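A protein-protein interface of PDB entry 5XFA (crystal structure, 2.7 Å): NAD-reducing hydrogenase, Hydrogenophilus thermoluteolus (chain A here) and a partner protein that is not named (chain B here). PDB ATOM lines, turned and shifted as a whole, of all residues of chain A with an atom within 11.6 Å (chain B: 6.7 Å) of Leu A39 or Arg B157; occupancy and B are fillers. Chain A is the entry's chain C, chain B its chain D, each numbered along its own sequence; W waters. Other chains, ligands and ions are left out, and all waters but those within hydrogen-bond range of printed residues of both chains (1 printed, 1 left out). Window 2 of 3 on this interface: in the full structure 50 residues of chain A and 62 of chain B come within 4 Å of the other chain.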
ATOM      1  N   LYS A  13      12.103  -7.154   8.189  1.00  0.00           N
ATOM      2  CA  LYS A  13      11.090  -7.952   8.898  1.00  0.00           C
ATOM      3  C   LYS A  13      10.162  -8.655   7.907  1.00  0.00           C
ATOM      4  O   LYS A  13       9.839  -8.099   6.864  1.00  0.00           O
ATOM      5  CB  LYS A  13      10.237  -7.066   9.819  1.00  0.00           C
ATOM      6  CG  LYS A  13      10.846  -6.732  11.175  1.00  0.00           C
ATOM      7  CD  LYS A  13       9.766  -6.291  12.157  1.00  0.00           C
ATOM      8  CE  LYS A  13      10.347  -5.600  13.374  1.00  0.00           C
ATOM      9  NZ  LYS A  13      10.617  -4.161  13.138  1.00  0.00           N
ATOM     10  N   PHE A  31      -5.167 -18.049  16.780  1.00  0.00           N
ATOM     11  CA  PHE A  31      -3.911 -17.312  16.586  1.00  0.00           C
ATOM     12  C   PHE A  31      -3.593 -16.423  17.802  1.00  0.00           C
ATOM     13  O   PHE A  31      -2.531 -16.566  18.397  1.00  0.00           O
ATOM     14  CB  PHE A  31      -3.968 -16.476  15.301  1.00  0.00           C
ATOM     15  CG  PHE A  31      -2.863 -15.487  15.171  1.00  0.00           C
ATOM     16  CD1 PHE A  31      -1.641 -15.864  14.635  1.00  0.00           C
ATOM     17  CD2 PHE A  31      -3.039 -14.181  15.580  1.00  0.00           C
ATOM     18  CE1 PHE A  31      -0.605 -14.956  14.509  1.00  0.00           C
ATOM     19  CE2 PHE A  31      -2.005 -13.273  15.461  1.00  0.00           C
ATOM     20  CZ  PHE A  31      -0.787 -13.661  14.926  1.00  0.00           C
ATOM     21  N   ALA A  32      -4.518 -15.540  18.186  1.00  0.00           N
ATOM     22  CA  ALA A  32      -4.329 -14.695  19.378  1.00  0.00           C
ATOM     23  C   ALA A  32      -4.139 -15.493  20.674  1.00  0.00           C
ATOM     24  O   ALA A  32      -3.636 -14.949  21.670  1.00  0.00           O
ATOM     25  CB  ALA A  32      -5.490 -13.735  19.552  1.00  0.00           C
ATOM     26  N   ASP A  33      -4.544 -16.769  20.666  1.00  0.00           N
ATOM     27  CA  ASP A  33      -4.322 -17.685  21.815  1.00  0.00           C
ATOM     28  C   ASP A  33      -2.865 -18.044  22.075  1.00  0.00           C
ATOM     29  O   ASP A  33      -2.555 -18.590  23.118  1.00  0.00           O
ATOM     30  CB  ASP A  33      -5.123 -18.998  21.677  1.00  0.00           C
ATOM     31  CG  ASP A  33      -6.559 -18.877  22.149  1.00  0.00           C
ATOM     32  OD1 ASP A  33      -6.925 -17.837  22.790  1.00  0.00           O
ATOM     33  OD2 ASP A  33      -7.318 -19.844  21.863  1.00  0.00           O
ATOM     34  N   ILE A  34      -1.973 -17.709  21.157  1.00  0.00           N
ATOM     35  CA  ILE A  34      -0.555 -17.711  21.499  1.00  0.00           C
ATOM     36  C   ILE A  34      -0.185 -16.770  22.672  1.00  0.00           C
ATOM     37  O   ILE A  34       0.893 -16.896  23.241  1.00  0.00           O
ATOM     38  CB  ILE A  34       0.338 -17.392  20.286  1.00  0.00           C
ATOM     39  CG1 ILE A  34       0.267 -15.928  19.916  1.00  0.00           C
ATOM     40  CG2 ILE A  34       0.026 -18.343  19.117  1.00  0.00           C
ATOM     41  CD1 ILE A  34       1.183 -15.590  18.764  1.00  0.00           C
ATOM     42  N   ASP A  35      -1.083 -15.850  23.031  1.00  0.00           N
ATOM     43  CA  ASP A  35      -0.975 -15.046  24.254  1.00  0.00           C
ATOM     44  C   ASP A  35       0.225 -14.107  24.227  1.00  0.00           C
ATOM     45  O   ASP A  35       0.427 -13.396  23.246  1.00  0.00           O
ATOM     46  CB  ASP A  35      -1.011 -15.927  25.509  1.00  0.00           C
ATOM     47  CG  ASP A  35      -2.270 -16.748  25.600  1.00  0.00           C
ATOM     48  OD1 ASP A  35      -3.371 -16.161  25.504  1.00  0.00           O
ATOM     49  OD2 ASP A  35      -2.177 -17.991  25.767  1.00  0.00           O
ATOM     50  N   THR A  36       1.031 -14.071  25.274  1.00  0.00           N
ATOM     51  CA  THR A  36       2.069 -13.055  25.320  1.00  0.00           C
ATOM     52  C   THR A  36       3.072 -13.240  24.198  1.00  0.00           C
ATOM     53  O   THR A  36       3.795 -12.300  23.858  1.00  0.00           O
ATOM     54  CB  THR A  36       2.779 -13.022  26.672  1.00  0.00           C
ATOM     55  OG1 THR A  36       3.003 -14.353  27.137  1.00  0.00           O
ATOM     56  CG2 THR A  36       1.900 -12.310  27.685  1.00  0.00           C
ATOM     57  N   ARG A  37       3.117 -14.433  23.617  1.00  0.00           N
ATOM     58  CA  ARG A  37       4.010 -14.705  22.502  1.00  0.00           C
ATOM     59  C   ARG A  37       3.748 -13.795  21.309  1.00  0.00           C
ATOM     60  O   ARG A  37       4.604 -13.632  20.440  1.00  0.00           O
ATOM     61  CB  ARG A  37       3.886 -16.167  22.058  1.00  0.00           C
ATOM     62  CG  ARG A  37       4.471 -17.119  23.079  1.00  0.00           C
ATOM     63  CD  ARG A  37       4.340 -18.551  22.650  1.00  0.00           C
ATOM     64  NE  ARG A  37       3.003 -19.064  22.892  1.00  0.00           N
ATOM     65  CZ  ARG A  37       2.605 -20.288  22.551  1.00  0.00           C
ATOM     66  NH1 ARG A  37       3.450 -21.127  21.949  1.00  0.00           N
ATOM     67  NH2 ARG A  37       1.365 -20.674  22.806  1.00  0.00           N
ATOM     68  N   LEU A  38       2.553 -13.217  21.254  1.00  0.00           N
ATOM     69  CA  LEU A  38       2.231 -12.256  20.225  1.00  0.00           C
ATOM     70  C   LEU A  38       3.135 -11.016  20.376  1.00  0.00           C
ATOM     71  O   LEU A  38       3.401 -10.316  19.399  1.00  0.00           O
ATOM     72  CB  LEU A  38       0.755 -11.882  20.324  1.00  0.00           C
ATOM     73  CG  LEU A  38       0.228 -10.884  19.294  1.00  0.00           C
ATOM     74  CD1 LEU A  38       0.051 -11.547  17.945  1.00  0.00           C
ATOM     75  CD2 LEU A  38      -1.078 -10.281  19.757  1.00  0.00           C
ATOM     76  N   LEU A  39       3.609 -10.737  21.584  1.00  0.00           N
ATOM     77  CA  LEU A  39       4.515  -9.599  21.787  1.00  0.00           C
ATOM     78  C   LEU A  39       5.845  -9.896  21.141  1.00  0.00           C
ATOM     79  O   LEU A  39       6.471  -9.002  20.572  1.00  0.00           O
ATOM     80  CB  LEU A  39       4.729  -9.285  23.273  1.00  0.00           C
ATOM     81  CG  LEU A  39       3.484  -8.886  24.069  1.00  0.00           C
ATOM     82  CD1 LEU A  39       3.826  -8.631  25.535  1.00  0.00           C
ATOM     83  CD2 LEU A  39       2.816  -7.676  23.437  1.00  0.00           C
ATOM     84  N   ALA A  40       6.282 -11.147  21.250  1.00  0.00           N
ATOM     85  CA  ALA A  40       7.513 -11.576  20.595  1.00  0.00           C
ATOM     86  C   ALA A  40       7.330 -11.632  19.089  1.00  0.00           C
ATOM     87  O   ALA A  40       8.231 -11.330  18.344  1.00  0.00           O
ATOM     88  CB  ALA A  40       7.970 -12.918  21.126  1.00  0.00           C
ATOM     89  N   LEU A  41       6.143 -11.971  18.644  1.00  0.00           N
ATOM     90  CA  LEU A  41       5.871 -12.009  17.219  1.00  0.00           C
ATOM     91  C   LEU A  41       5.891 -10.623  16.624  1.00  0.00           C
ATOM     92  O   LEU A  41       6.363 -10.443  15.502  1.00  0.00           O
ATOM     93  CB  LEU A  41       4.529 -12.674  16.944  1.00  0.00           C
ATOM     94  CG  LEU A  41       4.374 -13.101  15.494  1.00  0.00           C
ATOM     95  CD1 LEU A  41       5.366 -14.199  15.146  1.00  0.00           C
ATOM     96  CD2 LEU A  41       2.959 -13.590  15.233  1.00  0.00           C
ATOM     97  N   ALA A  42       5.387  -9.650  17.389  1.00  0.00           N
ATOM     98  CA  ALA A  42       5.348  -8.226  16.984  1.00  0.00           C
ATOM     99  C   ALA A  42       6.726  -7.676  16.652  1.00  0.00           C
ATOM    100  O   ALA A  42       6.875  -6.932  15.697  1.00  0.00           O
ATOM    101  CB  ALA A  42       4.689  -7.374  18.068  1.00  0.00           C
ATOM    102  N   GLU A  43       7.734  -8.073  17.422  1.00  0.00           N
ATOM    103  CA  GLU A  43       9.118  -7.709  17.139  1.00  0.00           C
ATOM    104  C   GLU A  43       9.639  -8.305  15.821  1.00  0.00           C
ATOM    105  O   GLU A  43      10.467  -7.682  15.169  1.00  0.00           O
ATOM    106  CB  GLU A  43      10.044  -8.178  18.272  1.00  0.00           C
ATOM    107  CG  GLU A  43       9.785  -7.598  19.656  1.00  0.00           C
ATOM    108  CD  GLU A  43      10.766  -8.160  20.700  1.00  0.00           C
ATOM    109  OE1 GLU A  43      10.853  -7.575  21.801  1.00  0.00           O
ATOM    110  OE2 GLU A  43      11.460  -9.184  20.434  1.00  0.00           O
ATOM    111  N   TRP A  44       9.211  -9.528  15.467  1.00  0.00           N
ATOM    112  CA  TRP A  44       9.783 -10.248  14.311  1.00  0.00           C
ATOM    113  C   TRP A  44       9.038 -10.036  13.005  1.00  0.00           C
ATOM    114  O   TRP A  44       9.596 -10.309  11.943  1.00  0.00           O
ATOM    115  CB  TRP A  44       9.880 -11.761  14.554  1.00  0.00           C
ATOM    116  CG  TRP A  44      10.610 -12.157  15.805  1.00  0.00           C
ATOM    117  CD1 TRP A  44      11.680 -11.525  16.366  1.00  0.00           C
ATOM    118  CD2 TRP A  44      10.325 -13.294  16.647  1.00  0.00           C
ATOM    119  NE1 TRP A  44      12.065 -12.180  17.517  1.00  0.00           N
ATOM    120  CE2 TRP A  44      11.252 -13.266  17.712  1.00  0.00           C
ATOM    121  CE3 TRP A  44       9.366 -14.320  16.611  1.00  0.00           C
ATOM    122  CZ2 TRP A  44      11.256 -14.230  18.727  1.00  0.00           C
ATOM    123  CZ3 TRP A  44       9.369 -15.277  17.625  1.00  0.00           C
ATOM    124  CH2 TRP A  44      10.311 -15.227  18.664  1.00  0.00           C
ATOM    125  N   VAL A  45       7.784  -9.587  13.060  1.00  0.00           N
ATOM    126  CA  VAL A  45       7.027  -9.418  11.828  1.00  0.00           C
ATOM    127  C   VAL A  45       6.254  -8.110  11.762  1.00  0.00           C
ATOM    128  O   VAL A  45       6.207  -7.328  12.714  1.00  0.00           O
ATOM    129  CB  VAL A  45       6.047 -10.585  11.586  1.00  0.00           C
ATOM    130  CG1 VAL A  45       6.709 -11.929  11.861  1.00  0.00           C
ATOM    131  CG2 VAL A  45       4.783 -10.421  12.416  1.00  0.00           C
ATOM    132  N   THR A  46       5.650  -7.904  10.598  1.00  0.00           N
ATOM    133  CA  THR A  46       4.877  -6.723  10.292  1.00  0.00           C
ATOM    134  C   THR A  46       3.619  -7.169   9.540  1.00  0.00           C
ATOM    135  O   THR A  46       3.689  -8.026   8.661  1.00  0.00           O
ATOM    136  CB  THR A  46       5.718  -5.768   9.439  1.00  0.00           C
ATOM    137  OG1 THR A  46       6.878  -5.386  10.184  1.00  0.00           O
ATOM    138  CG2 THR A  46       4.933  -4.519   9.054  1.00  0.00           C
ATOM    139  N   PHE A  47       2.475  -6.590   9.896  1.00  0.00           N
ATOM    140  CA  PHE A  47       1.189  -7.012   9.352  1.00  0.00           C
ATOM    141  C   PHE A  47       0.636  -6.086   8.292  1.00  0.00           C
ATOM    142  O   PHE A  47       0.524  -4.865   8.483  1.00  0.00           O
ATOM    143  CB  PHE A  47       0.195  -7.187  10.484  1.00  0.00           C
ATOM    144  CG  PHE A  47       0.527  -8.352  11.355  1.00  0.00           C
ATOM    145  CD1 PHE A  47       1.399  -8.204  12.429  1.00  0.00           C
ATOM    146  CD2 PHE A  47       0.029  -9.638  11.048  1.00  0.00           C
ATOM    147  CE1 PHE A  47       1.723  -9.300  13.217  1.00  0.00           C
ATOM    148  CE2 PHE A  47       0.351 -10.732  11.829  1.00  0.00           C
ATOM    149  CZ  PHE A  47       1.197 -10.567  12.914  1.00  0.00           C
ATOM    150  N   LEU A  52      -7.192  -7.344  12.179  1.00  0.00           N
ATOM    151  CA  LEU A  52      -6.541  -6.663  13.301  1.00  0.00           C
ATOM    152  C   LEU A  52      -5.883  -5.272  12.981  1.00  0.00           C
ATOM    153  O   LEU A  52      -5.492  -4.530  13.897  1.00  0.00           O
ATOM    154  CB  LEU A  52      -5.483  -7.593  13.870  1.00  0.00           C
ATOM    155  CG  LEU A  52      -5.935  -8.938  14.426  1.00  0.00           C
ATOM    156  CD1 LEU A  52      -4.734  -9.656  15.042  1.00  0.00           C
ATOM    157  CD2 LEU A  52      -7.037  -8.737  15.455  1.00  0.00           C
ATOM    158  N   TRP A 167       1.479 -21.522  16.312  1.00  0.00           N
ATOM    159  CA  TRP A 167       2.795 -21.041  16.717  1.00  0.00           C
ATOM    160  C   TRP A 167       3.922 -21.812  16.069  1.00  0.00           C
ATOM    161  O   TRP A 167       4.873 -21.229  15.551  1.00  0.00           O
ATOM    162  CB  TRP A 167       2.970 -21.157  18.214  1.00  0.00           C
ATOM    163  CG  TRP A 167       4.215 -20.541  18.681  1.00  0.00           C
ATOM    164  CD1 TRP A 167       5.262 -21.171  19.262  1.00  0.00           C
ATOM    165  CD2 TRP A 167       4.565 -19.158  18.608  1.00  0.00           C
ATOM    166  NE1 TRP A 167       6.241 -20.262  19.590  1.00  0.00           N
ATOM    167  CE2 TRP A 167       5.842 -19.018  19.192  1.00  0.00           C
ATOM    168  CE3 TRP A 167       3.915 -18.013  18.126  1.00  0.00           C
ATOM    169  CZ2 TRP A 167       6.486 -17.786  19.306  1.00  0.00           C
ATOM    170  CZ3 TRP A 167       4.562 -16.783  18.233  1.00  0.00           C
ATOM    171  CH2 TRP A 167       5.833 -16.684  18.816  1.00  0.00           C
ATOM    172  N   LEU A 170       4.372 -20.879  12.353  1.00  0.00           N
ATOM    173  CA  LEU A 170       5.045 -19.598  12.122  1.00  0.00           C
ATOM    174  C   LEU A 170       6.522 -19.675  12.518  1.00  0.00           C
ATOM    175  O   LEU A 170       7.402 -19.387  11.714  1.00  0.00           O
ATOM    176  CB  LEU A 170       4.350 -18.457  12.882  1.00  0.00           C
ATOM    177  CG  LEU A 170       2.918 -18.131  12.440  1.00  0.00           C
ATOM    178  CD1 LEU A 170       2.259 -17.092  13.330  1.00  0.00           C
ATOM    179  CD2 LEU A 170       2.900 -17.676  10.988  1.00  0.00           C
ATOM    180  N   LEU A 174       9.488 -18.685   9.895  1.00  0.00           N
ATOM    181  CA  LEU A 174      10.380 -17.553  10.171  1.00  0.00           C
ATOM    182  C   LEU A 174      11.846 -17.963  10.092  1.00  0.00           C
ATOM    183  O   LEU A 174      12.669 -17.238   9.538  1.00  0.00           O
ATOM    184  CB  LEU A 174      10.090 -16.960  11.545  1.00  0.00           C
ATOM    185  CG  LEU A 174       8.692 -16.361  11.722  1.00  0.00           C
ATOM    186  CD1 LEU A 174       8.367 -16.225  13.201  1.00  0.00           C
ATOM    187  CD2 LEU A 174       8.567 -15.025  11.009  1.00  0.00           C
ATOM    188  N   VAL B 149      -3.003  -3.449  17.444  1.00  0.00           N
ATOM    189  CA  VAL B 149      -2.576  -4.062  18.690  1.00  0.00           C
ATOM    190  C   VAL B 149      -1.052  -4.186  18.802  1.00  0.00           C
ATOM    191  O   VAL B 149      -0.518  -4.306  19.908  1.00  0.00           O
ATOM    192  CB  VAL B 149      -3.298  -5.419  18.884  1.00  0.00           C
ATOM    193  CG1 VAL B 149      -2.820  -6.467  17.885  1.00  0.00           C
ATOM    194  CG2 VAL B 149      -3.140  -5.923  20.316  1.00  0.00           C
ATOM    195  N   LEU B 152       0.439  -0.863  19.745  1.00  0.00           N
ATOM    196  CA  LEU B 152       0.147  -0.760  21.174  1.00  0.00           C
ATOM    197  C   LEU B 152       1.129  -1.591  22.005  1.00  0.00           C
ATOM    198  O   LEU B 152       1.618  -1.148  23.052  1.00  0.00           O
ATOM    199  CB  LEU B 152      -1.275  -1.241  21.428  1.00  0.00           C
ATOM    200  CG  LEU B 152      -1.892  -0.881  22.771  1.00  0.00           C
ATOM    201  CD1 LEU B 152      -2.105   0.620  22.875  1.00  0.00           C
ATOM    202  CD2 LEU B 152      -3.208  -1.613  22.958  1.00  0.00           C
ATOM    203  N   ALA B 153       1.413  -2.803  21.529  1.00  0.00           N
ATOM    204  CA  ALA B 153       2.406  -3.675  22.160  1.00  0.00           C
ATOM    205  C   ALA B 153       3.780  -2.994  22.231  1.00  0.00           C
ATOM    206  O   ALA B 153       4.465  -3.068  23.244  1.00  0.00           O
ATOM    207  CB  ALA B 153       2.517  -4.983  21.396  1.00  0.00           C
ATOM    208  N   ALA B 154       4.158  -2.325  21.143  1.00  0.00           N
ATOM    209  CA  ALA B 154       5.414  -1.583  21.062  1.00  0.00           C
ATOM    210  C   ALA B 154       5.469  -0.371  22.015  1.00  0.00           C
ATOM    211  O   ALA B 154       6.479  -0.133  22.681  1.00  0.00           O
ATOM    212  CB  ALA B 154       5.634  -1.128  19.628  1.00  0.00           C
ATOM    213  N   GLN B 155       4.378   0.388  22.076  1.00  0.00           N
ATOM    214  CA  GLN B 155       4.349   1.637  22.834  1.00  0.00           C
ATOM    215  C   GLN B 155       3.977   1.419  24.289  1.00  0.00           C
ATOM    216  O   GLN B 155       4.714   1.823  25.175  1.00  0.00           O
ATOM    217  CB  GLN B 155       3.391   2.615  22.166  1.00  0.00           C
ATOM    218  CG  GLN B 155       3.862   3.006  20.767  1.00  0.00           C
ATOM    219  CD  GLN B 155       3.022   4.092  20.121  1.00  0.00           C
ATOM    220  OE1 GLN B 155       2.629   3.974  18.955  1.00  0.00           O
ATOM    221  NE2 GLN B 155       2.763   5.174  20.866  1.00  0.00           N
ATOM    222  N   LYS B 156       2.855   0.751  24.527  1.00  0.00           N
ATOM    223  CA  LYS B 156       2.308   0.578  25.871  1.00  0.00           C
ATOM    224  C   LYS B 156       2.302  -0.899  26.219  1.00  0.00           C
ATOM    225  O   LYS B 156       1.255  -1.531  26.399  1.00  0.00           O
ATOM    226  CB  LYS B 156       0.901   1.168  25.930  1.00  0.00           C
ATOM    227  CG  LYS B 156       0.800   2.531  25.251  1.00  0.00           C
ATOM    228  CD  LYS B 156      -0.079   3.515  26.007  1.00  0.00           C
ATOM    229  CE  LYS B 156       0.186   4.934  25.533  1.00  0.00           C
ATOM    230  NZ  LYS B 156      -0.537   5.918  26.378  1.00  0.00           N
ATOM    231  N   ARG B 157       3.505  -1.434  26.333  1.00  0.00           N
ATOM    232  CA  ARG B 157       3.702  -2.865  26.402  1.00  0.00           C
ATOM    233  C   ARG B 157       3.081  -3.485  27.641  1.00  0.00           C
ATOM    234  O   ARG B 157       2.342  -4.459  27.550  1.00  0.00           O
ATOM    235  CB  ARG B 157       5.191  -3.180  26.381  1.00  0.00           C
ATOM    236  CG  ARG B 157       5.507  -4.656  26.281  1.00  0.00           C
ATOM    237  CD  ARG B 157       6.952  -4.902  26.662  1.00  0.00           C
ATOM    238  NE  ARG B 157       7.279  -6.325  26.704  1.00  0.00           N
ATOM    239  CZ  ARG B 157       7.412  -7.112  25.634  1.00  0.00           C
ATOM    240  NH1 ARG B 157       7.235  -6.636  24.403  1.00  0.00           N
ATOM    241  NH2 ARG B 157       7.724  -8.393  25.799  1.00  0.00           N
ATOM    242  N   GLU B 158       3.394  -2.948  28.806  1.00  0.00           N
ATOM    243  CA  GLU B 158       2.931  -3.565  30.038  1.00  0.00           C
ATOM    244  C   GLU B 158       1.403  -3.526  30.111  1.00  0.00           C
ATOM    245  O   GLU B 158       0.784  -4.314  30.823  1.00  0.00           O
ATOM    246  CB  GLU B 158       3.580  -2.880  31.245  1.00  0.00           C
ATOM    247  CG  GLU B 158       3.098  -3.345  32.610  1.00  0.00           C
ATOM    248  CD  GLU B 158       3.150  -4.850  32.807  1.00  0.00           C
ATOM    249  OE1 GLU B 158       4.030  -5.509  32.206  1.00  0.00           O
ATOM    250  OE2 GLU B 158       2.305  -5.362  33.578  1.00  0.00           O
ATOM    251  N   LEU B 159       0.794  -2.592  29.393  1.00  0.00           N
ATOM    252  CA  LEU B 159      -0.644  -2.521  29.365  1.00  0.00           C
ATOM    253  C   LEU B 159      -1.161  -3.654  28.511  1.00  0.00           C
ATOM    254  O   LEU B 159      -1.914  -4.491  28.978  1.00  0.00           O
ATOM    255  CB  LEU B 159      -1.111  -1.194  28.806  1.00  0.00           C
ATOM    256  CG  LEU B 159      -2.455  -0.798  29.382  1.00  0.00           C
ATOM    257  CD1 LEU B 159      -2.248  -0.025  30.687  1.00  0.00           C
ATOM    258  CD2 LEU B 159      -3.226   0.012  28.353  1.00  0.00           C
ATOM    259  N   ALA B 160      -0.717  -3.704  27.267  1.00  0.00           N
ATOM    260  CA  ALA B 160      -1.079  -4.804  26.366  1.00  0.00           C
ATOM    261  C   ALA B 160      -0.781  -6.221  26.911  1.00  0.00           C
ATOM    262  O   ALA B 160      -1.526  -7.145  26.635  1.00  0.00           O
ATOM    263  CB  ALA B 160      -0.399  -4.624  25.007  1.00  0.00           C
ATOM    264  N   ARG B 161       0.305  -6.389  27.659  1.00  0.00           N
ATOM    265  CA  ARG B 161       0.599  -7.668  28.293  1.00  0.00           C
ATOM    266  C   ARG B 161      -0.488  -8.039  29.309  1.00  0.00           C
ATOM    267  O   ARG B 161      -0.885  -9.195  29.414  1.00  0.00           O
ATOM    268  CB  ARG B 161       1.960  -7.636  28.970  1.00  0.00           C
ATOM    269  CG  ARG B 161       2.460  -8.969  29.488  1.00  0.00           C
ATOM    270  CD  ARG B 161       3.754  -8.813  30.288  1.00  0.00           C
ATOM    271  NE  ARG B 161       3.742  -9.619  31.509  1.00  0.00           N
ATOM    272  CZ  ARG B 161       3.154  -9.262  32.644  1.00  0.00           C
ATOM    273  NH1 ARG B 161       2.531  -8.096  32.758  1.00  0.00           N
ATOM    274  NH2 ARG B 161       3.179 -10.074  33.688  1.00  0.00           N
ATOM    275  N   GLN B 162      -0.979  -7.065  30.048  1.00  0.00           N
ATOM    276  CA  GLN B 162      -2.043  -7.335  31.001  1.00  0.00           C
ATOM    277  C   GLN B 162      -3.300  -7.794  30.300  1.00  0.00           C
ATOM    278  O   GLN B 162      -3.893  -8.780  30.702  1.00  0.00           O
ATOM    279  CB  GLN B 162      -2.339  -6.094  31.841  1.00  0.00           C
ATOM    280  CG  GLN B 162      -1.226  -5.807  32.825  1.00  0.00           C
ATOM    281  CD  GLN B 162      -1.413  -4.512  33.556  1.00  0.00           C
ATOM    282  OE1 GLN B 162      -2.364  -3.748  33.308  1.00  0.00           O
ATOM    283  NE2 GLN B 162      -0.503  -4.249  34.477  1.00  0.00           N
ATOM    284  N   ILE B 164      -3.770  -9.105  27.337  1.00  0.00           N
ATOM    285  CA  ILE B 164      -3.565 -10.416  26.771  1.00  0.00           C
ATOM    286  C   ILE B 164      -3.729 -11.426  27.864  1.00  0.00           C
ATOM    287  O   ILE B 164      -4.455 -12.382  27.702  1.00  0.00           O
ATOM    288  CB  ILE B 164      -2.169 -10.568  26.166  1.00  0.00           C
ATOM    289  CG1 ILE B 164      -2.043  -9.696  24.918  1.00  0.00           C
ATOM    290  CG2 ILE B 164      -1.928 -12.026  25.765  1.00  0.00           C
ATOM    291  CD1 ILE B 164      -0.616  -9.397  24.526  1.00  0.00           C
HETATM  292  O   HOH W   1      -5.070  -4.656  16.502  1.00  0.00           O
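The backbone carbonyl oxygen (O) of Asp A33 sits close to the side-chain carboxylate (OD2) of Asp A35, at 2.7 Å.
The side-chain carboxylate (OE2) of Glu B158 lies within salt-bridge range of the guanidinium group (NH1) of Arg B161, at 2.9 Å.
Asp A35 touches Ile B164.
Arg B161 touches Thr A36.
Thr A36 touches Ile B164 (N to CG2, 3.6 Å).
CB of Ala B153 touches CD2 of Leu A39 (3.4 Å).
NH1 of Arg B157 touches CB of Leu A39, 3.8 Å away.
Ile B164 touches Leu A39.
Among the printed residues, 6 pairs touch across the chains.
Among the printed residues, no Asp or Glu carboxylate lies within 4 Å of a Lys or Arg side-chain nitrogen of the other chain.
Of the printed residues of chain B, Leu A39 touches Ala B153 (3.4 Å), Arg B157 (3.8 Å) and Ile B164 (3.99 Å).
Arg B157 touches one residue of chain A.
No residue of chain A comes within 4 Å of Leu B152.
Ala B153 touches just one residue of chain A: Leu A39.
Glu B158 touches none of the printed residues of chain A.
No residue of chain A comes within 4 Å of Leu B159.
Ala B160 touches none of the printed residues of chain A.
Printed residues of chain B within 4 Å of Asp A35: Ile B164.
Of the printed residues of chain A, Ile B164 touches Asp A35, Thr A36 and Leu A39.
Of the printed residues of chain B, Thr A36 touches Arg B161 and Ile B164.
The nearest printed residue of chain A that does not touch Ile B164 is Leu A38 (4.9 Å).
Water W1 bridges N of Val B149 and O of Leu A52.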
